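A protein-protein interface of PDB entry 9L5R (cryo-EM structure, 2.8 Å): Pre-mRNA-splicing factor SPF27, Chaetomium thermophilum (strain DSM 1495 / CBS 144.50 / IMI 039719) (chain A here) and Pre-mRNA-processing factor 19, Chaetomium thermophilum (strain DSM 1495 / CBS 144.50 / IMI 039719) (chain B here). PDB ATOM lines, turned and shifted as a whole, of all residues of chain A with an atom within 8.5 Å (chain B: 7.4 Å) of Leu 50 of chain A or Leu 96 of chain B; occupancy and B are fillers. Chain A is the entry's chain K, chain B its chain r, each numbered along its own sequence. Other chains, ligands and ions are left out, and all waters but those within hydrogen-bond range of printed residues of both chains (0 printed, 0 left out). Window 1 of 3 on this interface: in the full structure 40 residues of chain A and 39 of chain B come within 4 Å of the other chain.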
ATOM      1  N   PRO A  47      -6.629  14.340  22.576  1.00  0.00           N
ATOM      2  CA  PRO A  47      -7.470  14.812  21.469  1.00  0.00           C
ATOM      3  C   PRO A  47      -7.582  16.326  21.483  1.00  0.00           C
ATOM      4  O   PRO A  47      -7.316  16.960  22.516  1.00  0.00           O
ATOM      5  CB  PRO A  47      -8.829  14.146  21.746  1.00  0.00           C
ATOM      6  CG  PRO A  47      -8.782  13.716  23.171  1.00  0.00           C
ATOM      7  CD  PRO A  47      -7.353  13.440  23.486  1.00  0.00           C
ATOM      8  N   PRO A  48      -7.932  16.939  20.352  1.00  0.00           N
ATOM      9  CA  PRO A  48      -8.093  18.392  20.328  1.00  0.00           C
ATOM     10  C   PRO A  48      -9.223  18.826  21.236  1.00  0.00           C
ATOM     11  O   PRO A  48     -10.208  18.088  21.432  1.00  0.00           O
ATOM     12  CB  PRO A  48      -8.405  18.690  18.854  1.00  0.00           C
ATOM     13  CG  PRO A  48      -8.829  17.386  18.267  1.00  0.00           C
ATOM     14  CD  PRO A  48      -8.051  16.354  19.005  1.00  0.00           C
ATOM     15  N   PRO A  49      -9.120  20.015  21.829  1.00  0.00           N
ATOM     16  CA  PRO A  49     -10.113  20.436  22.821  1.00  0.00           C
ATOM     17  C   PRO A  49     -11.450  20.782  22.188  1.00  0.00           C
ATOM     18  O   PRO A  49     -11.569  20.998  20.979  1.00  0.00           O
ATOM     19  CB  PRO A  49      -9.473  21.670  23.465  1.00  0.00           C
ATOM     20  CG  PRO A  49      -8.565  22.205  22.417  1.00  0.00           C
ATOM     21  CD  PRO A  49      -8.051  21.013  21.658  1.00  0.00           C
ATOM     22  N   LEU A  50     -12.468  20.817  23.037  1.00  0.00           N
ATOM     23  CA  LEU A  50     -13.814  21.163  22.603  1.00  0.00           C
ATOM     24  C   LEU A  50     -13.861  22.634  22.214  1.00  0.00           C
ATOM     25  O   LEU A  50     -13.514  23.493  23.035  1.00  0.00           O
ATOM     26  CB  LEU A  50     -14.816  20.878  23.717  1.00  0.00           C
ATOM     27  CG  LEU A  50     -14.660  19.549  24.459  1.00  0.00           C
ATOM     28  CD1 LEU A  50     -15.631  19.474  25.625  1.00  0.00           C
ATOM     29  CD2 LEU A  50     -14.861  18.373  23.516  1.00  0.00           C
ATOM     30  N   PRO A  51     -14.254  22.970  20.988  1.00  0.00           N
ATOM     31  CA  PRO A  51     -14.324  24.378  20.586  1.00  0.00           C
ATOM     32  C   PRO A  51     -15.447  25.097  21.311  1.00  0.00           C
ATOM     33  O   PRO A  51     -16.484  24.492  21.622  1.00  0.00           O
ATOM     34  CB  PRO A  51     -14.593  24.300  19.077  1.00  0.00           C
ATOM     35  CG  PRO A  51     -15.261  22.984  18.885  1.00  0.00           C
ATOM     36  CD  PRO A  51     -14.651  22.061  19.900  1.00  0.00           C
ATOM     37  N   PRO A  52     -15.274  26.389  21.610  1.00  0.00           N
ATOM     38  CA  PRO A  52     -16.365  27.153  22.234  1.00  0.00           C
ATOM     39  C   PRO A  52     -17.542  27.383  21.296  1.00  0.00           C
ATOM     40  O   PRO A  52     -17.490  27.043  20.110  1.00  0.00           O
ATOM     41  CB  PRO A  52     -15.693  28.472  22.639  1.00  0.00           C
ATOM     42  CG  PRO A  52     -14.406  28.520  21.885  1.00  0.00           C
ATOM     43  CD  PRO A  52     -13.990  27.106  21.668  1.00  0.00           C
ATOM     44  N   LEU A  53     -18.613  27.970  21.831  1.00  0.00           N
ATOM     45  CA  LEU A  53     -19.889  28.005  21.126  1.00  0.00           C
ATOM     46  C   LEU A  53     -19.920  29.031  19.998  1.00  0.00           C
ATOM     47  O   LEU A  53     -20.618  28.819  19.001  1.00  0.00           O
ATOM     48  CB  LEU A  53     -21.016  28.297  22.118  1.00  0.00           C
ATOM     49  CG  LEU A  53     -20.981  27.515  23.434  1.00  0.00           C
ATOM     50  CD1 LEU A  53     -21.793  28.231  24.505  1.00  0.00           C
ATOM     51  CD2 LEU A  53     -21.466  26.085  23.252  1.00  0.00           C
ATOM     52  N   GLU A  55     -17.695  30.477  17.686  1.00  0.00           N
ATOM     53  CA  GLU A  55     -17.099  30.296  16.369  1.00  0.00           C
ATOM     54  C   GLU A  55     -17.633  29.069  15.644  1.00  0.00           C
ATOM     55  O   GLU A  55     -17.360  28.904  14.449  1.00  0.00           O
ATOM     56  CB  GLU A  55     -15.571  30.210  16.487  1.00  0.00           C
ATOM     57  CG  GLU A  55     -15.009  28.799  16.632  1.00  0.00           C
ATOM     58  CD  GLU A  55     -14.885  28.360  18.073  1.00  0.00           C
ATOM     59  OE1 GLU A  55     -15.611  28.908  18.926  1.00  0.00           O
ATOM     60  OE2 GLU A  55     -14.056  27.470  18.354  1.00  0.00           O
ATOM     61  N   TYR B  90     -27.346  21.059  26.944  1.00  0.00           N
ATOM     62  CA  TYR B  90     -26.499  21.738  27.920  1.00  0.00           C
ATOM     63  C   TYR B  90     -25.765  20.737  28.808  1.00  0.00           C
ATOM     64  O   TYR B  90     -24.528  20.766  28.905  1.00  0.00           O
ATOM     65  CB  TYR B  90     -27.362  22.682  28.758  1.00  0.00           C
ATOM     66  CG  TYR B  90     -26.625  23.500  29.791  1.00  0.00           C
ATOM     67  CD1 TYR B  90     -25.982  24.680  29.442  1.00  0.00           C
ATOM     68  CD2 TYR B  90     -26.605  23.112  31.126  1.00  0.00           C
ATOM     69  CE1 TYR B  90     -25.321  25.440  30.389  1.00  0.00           C
ATOM     70  CE2 TYR B  90     -25.948  23.864  32.079  1.00  0.00           C
ATOM     71  CZ  TYR B  90     -25.308  25.027  31.705  1.00  0.00           C
ATOM     72  OH  TYR B  90     -24.651  25.778  32.652  1.00  0.00           O
ATOM     73  N   THR B  91     -26.515  19.813  29.421  1.00  0.00           N
ATOM     74  CA  THR B  91     -25.916  18.825  30.312  1.00  0.00           C
ATOM     75  C   THR B  91     -24.930  17.938  29.569  1.00  0.00           C
ATOM     76  O   THR B  91     -23.899  17.554  30.127  1.00  0.00           O
ATOM     77  CB  THR B  91     -27.003  17.978  30.974  1.00  0.00           C
ATOM     78  OG1 THR B  91     -27.918  17.507  29.977  1.00  0.00           O
ATOM     79  CG2 THR B  91     -27.757  18.795  32.010  1.00  0.00           C
ATOM     80  N   THR B  92     -25.210  17.645  28.292  1.00  0.00           N
ATOM     81  CA  THR B  92     -24.265  16.918  27.454  1.00  0.00           C
ATOM     82  C   THR B  92     -22.970  17.700  27.280  1.00  0.00           C
ATOM     83  O   THR B  92     -21.877  17.122  27.339  1.00  0.00           O
ATOM     84  CB  THR B  92     -24.899  16.622  26.092  1.00  0.00           C
ATOM     85  OG1 THR B  92     -26.166  15.981  26.282  1.00  0.00           O
ATOM     86  CG2 THR B  92     -24.001  15.715  25.263  1.00  0.00           C
ATOM     87  N   ARG B  93     -23.077  19.018  27.089  1.00  0.00           N
ATOM     88  CA  ARG B  93     -21.887  19.843  26.900  1.00  0.00           C
ATOM     89  C   ARG B  93     -20.998  19.840  28.142  1.00  0.00           C
ATOM     90  O   ARG B  93     -19.786  19.587  28.051  1.00  0.00           O
ATOM     91  CB  ARG B  93     -22.296  21.269  26.531  1.00  0.00           C
ATOM     92  CG  ARG B  93     -21.138  22.154  26.113  1.00  0.00           C
ATOM     93  CD  ARG B  93     -20.885  22.027  24.621  1.00  0.00           C
ATOM     94  NE  ARG B  93     -19.803  21.098  24.320  1.00  0.00           N
ATOM     95  CZ  ARG B  93     -19.498  20.677  23.101  1.00  0.00           C
ATOM     96  NH1 ARG B  93     -20.189  21.065  22.042  1.00  0.00           N
ATOM     97  NH2 ARG B  93     -18.474  19.844  22.938  1.00  0.00           N
ATOM     98  N   GLU B  94     -21.582  20.091  29.323  1.00  0.00           N
ATOM     99  CA  GLU B  94     -20.721  20.064  30.512  1.00  0.00           C
ATOM    100  C   GLU B  94     -20.268  18.659  30.913  1.00  0.00           C
ATOM    101  O   GLU B  94     -19.172  18.525  31.470  1.00  0.00           O
ATOM    102  CB  GLU B  94     -21.304  20.786  31.741  1.00  0.00           C
ATOM    103  CG  GLU B  94     -21.267  22.329  31.707  1.00  0.00           C
ATOM    104  CD  GLU B  94     -22.449  23.009  31.078  1.00  0.00           C
ATOM    105  OE1 GLU B  94     -23.418  22.327  30.744  1.00  0.00           O
ATOM    106  OE2 GLU B  94     -22.397  24.245  30.911  1.00  0.00           O
ATOM    107  N   GLN B  95     -21.041  17.598  30.639  1.00  0.00           N
ATOM    108  CA  GLN B  95     -20.494  16.284  30.971  1.00  0.00           C
ATOM    109  C   GLN B  95     -19.374  15.903  30.012  1.00  0.00           C
ATOM    110  O   GLN B  95     -18.421  15.232  30.419  1.00  0.00           O
ATOM    111  CB  GLN B  95     -21.575  15.192  31.009  1.00  0.00           C
ATOM    112  CG  GLN B  95     -22.308  14.876  29.716  1.00  0.00           C
ATOM    113  CD  GLN B  95     -21.574  13.896  28.823  1.00  0.00           C
ATOM    114  OE1 GLN B  95     -20.835  13.034  29.299  1.00  0.00           O
ATOM    115  NE2 GLN B  95     -21.748  14.049  27.522  1.00  0.00           N
ATOM    116  N   LEU B  96     -19.459  16.333  28.747  1.00  0.00           N
ATOM    117  CA  LEU B  96     -18.351  16.125  27.821  1.00  0.00           C
ATOM    118  C   LEU B  96     -17.113  16.884  28.276  1.00  0.00           C
ATOM    119  O   LEU B  96     -15.996  16.357  28.194  1.00  0.00           O
ATOM    120  CB  LEU B  96     -18.760  16.544  26.409  1.00  0.00           C
ATOM    121  CG  LEU B  96     -17.721  16.389  25.293  1.00  0.00           C
ATOM    122  CD1 LEU B  96     -17.059  15.019  25.332  1.00  0.00           C
ATOM    123  CD2 LEU B  96     -18.357  16.628  23.937  1.00  0.00           C
ATOM    124  N   ALA B  97     -17.293  18.110  28.778  1.00  0.00           N
ATOM    125  CA  ALA B  97     -16.162  18.857  29.325  1.00  0.00           C
ATOM    126  C   ALA B  97     -15.550  18.150  30.533  1.00  0.00           C
ATOM    127  O   ALA B  97     -14.320  18.059  30.650  1.00  0.00           O
ATOM    128  CB  ALA B  97     -16.601  20.273  29.698  1.00  0.00           C
ATOM    129  N   ARG B  98     -16.394  17.629  31.431  1.00  0.00           N
ATOM    130  CA  ARG B  98     -15.895  16.938  32.619  1.00  0.00           C
ATOM    131  C   ARG B  98     -15.153  15.654  32.260  1.00  0.00           C
ATOM    132  O   ARG B  98     -14.094  15.363  32.831  1.00  0.00           O
ATOM    133  CB  ARG B  98     -17.051  16.634  33.572  1.00  0.00           C
ATOM    134  CG  ARG B  98     -17.618  17.854  34.275  1.00  0.00           C
ATOM    135  CD  ARG B  98     -18.537  17.454  35.417  1.00  0.00           C
ATOM    136  NE  ARG B  98     -19.692  16.693  34.955  1.00  0.00           N
ATOM    137  CZ  ARG B  98     -20.826  17.234  34.533  1.00  0.00           C
ATOM    138  NH1 ARG B  98     -20.991  18.547  34.485  1.00  0.00           N
ATOM    139  NH2 ARG B  98     -21.822  16.440  34.152  1.00  0.00           N
ATOM    140  N   VAL B  99     -15.691  14.874  31.320  1.00  0.00           N
ATOM    141  CA  VAL B  99     -15.029  13.637  30.918  1.00  0.00           C
ATOM    142  C   VAL B  99     -13.747  13.941  30.144  1.00  0.00           C
ATOM    143  O   VAL B  99     -12.766  13.195  30.243  1.00  0.00           O
ATOM    144  CB  VAL B  99     -16.015  12.745  30.133  1.00  0.00           C
ATOM    145  CG1 VAL B  99     -15.350  11.477  29.635  1.00  0.00           C
ATOM    146  CG2 VAL B  99     -17.180  12.352  31.025  1.00  0.00           C
ATOM    147  N   ARG B 100     -13.705  15.055  29.406  1.00  0.00           N
ATOM    148  CA  ARG B 100     -12.460  15.480  28.770  1.00  0.00           C
ATOM    149  C   ARG B 100     -11.398  15.850  29.804  1.00  0.00           C
ATOM    150  O   ARG B 100     -10.218  15.504  29.649  1.00  0.00           O
ATOM    151  CB  ARG B 100     -12.740  16.652  27.830  1.00  0.00           C
ATOM    152  CG  ARG B 100     -11.512  17.426  27.410  1.00  0.00           C
ATOM    153  CD  ARG B 100     -11.608  17.866  25.965  1.00  0.00           C
ATOM    154  NE  ARG B 100     -10.347  18.422  25.492  1.00  0.00           N
ATOM    155  CZ  ARG B 100      -9.305  17.698  25.102  1.00  0.00           C
ATOM    156  NH1 ARG B 100      -9.338  16.376  25.117  1.00  0.00           N
ATOM    157  NH2 ARG B 100      -8.204  18.316  24.687  1.00  0.00           N
ATOM    158  N   GLU B 101     -11.803  16.548  30.871  1.00  0.00           N
ATOM    159  CA  GLU B 101     -10.869  16.865  31.950  1.00  0.00           C
ATOM    160  C   GLU B 101     -10.368  15.600  32.639  1.00  0.00           C
ATOM    161  O   GLU B 101      -9.178  15.489  32.972  1.00  0.00           O
ATOM    162  CB  GLU B 101     -11.531  17.799  32.961  1.00  0.00           C
ATOM    163  CG  GLU B 101     -11.805  19.195  32.430  1.00  0.00           C
ATOM    164  CD  GLU B 101     -10.535  19.976  32.163  1.00  0.00           C
ATOM    165  OE1 GLU B 101      -9.560  19.807  32.925  1.00  0.00           O
ATOM    166  OE2 GLU B 101     -10.511  20.759  31.190  1.00  0.00           O
ATOM    167  N   GLU B 102     -11.263  14.632  32.859  1.00  0.00           N
ATOM    168  CA  GLU B 102     -10.852  13.351  33.425  1.00  0.00           C
ATOM    169  C   GLU B 102      -9.920  12.595  32.487  1.00  0.00           C
ATOM    170  O   GLU B 102      -9.014  11.892  32.948  1.00  0.00           O
ATOM    171  CB  GLU B 102     -12.080  12.502  33.754  1.00  0.00           C
ATOM    172  CG  GLU B 102     -12.849  12.980  34.975  1.00  0.00           C
ATOM    173  CD  GLU B 102     -12.090  12.746  36.267  1.00  0.00           C
ATOM    174  OE1 GLU B 102     -11.358  11.738  36.355  1.00  0.00           O
ATOM    175  OE2 GLU B 102     -12.222  13.574  37.193  1.00  0.00           O
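Pro 48 of chain A touches Arg 100 of chain B (C to NH2, 3.6 Å). CB of Leu 50 of chain A touches NH2 of Arg 93 of chain B, at 3.9 Å. CD1 of Leu 50 of chain A touches CG of Leu 96 of chain B, at 3.7 Å. Leu 50 of chain A touches Ala 97 of chain B. Leu 50 of chain A touches Arg 100 of chain B (CG to CD, 3.8 Å).
O of Pro 47 of chain A sits at hydrogen-bond distance from NH2 of Arg 100 of chain B (2.7 Å). NH2 of Arg 100 of chain B sits close to N of Pro 49 of chain A, 3.4 Å away.
Of the printed residues of chain B, Pro 47 of chain A touches Arg 100 (2.7 Å). Of the printed residues of chain B, Pro 48 of chain A touches Arg 100 (3.6 Å). Printed residues of chain B within 4 Å of Pro 49 of chain A: Arg 100. Of the printed residues of chain B, Leu 50 of chain A touches Arg 93, Leu 96, Ala 97 and Arg 100. Pro 51 of chain A touches none of the printed residues of chain B. No residue of chain A comes within 4 Å of Gln 95 of chain B. Of chain A, only Leu 50 comes within 4 Å of Leu 96 of chain B. Glu 101 of chain B touches none of the printed residues of chain A. The nearest residue of chain A that does not touch Leu 96 of chain B is Pro 51 of chain A (7.7 Å).
Of the 8 printed residues of chain A, 4 touch a printed residue of chain B. Printed residues of chain B that touch a printed residue of chain A: Arg 93, Leu 96, Ala 97 and Arg 100. Among the printed residues, 7 pairs touch across the chains.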
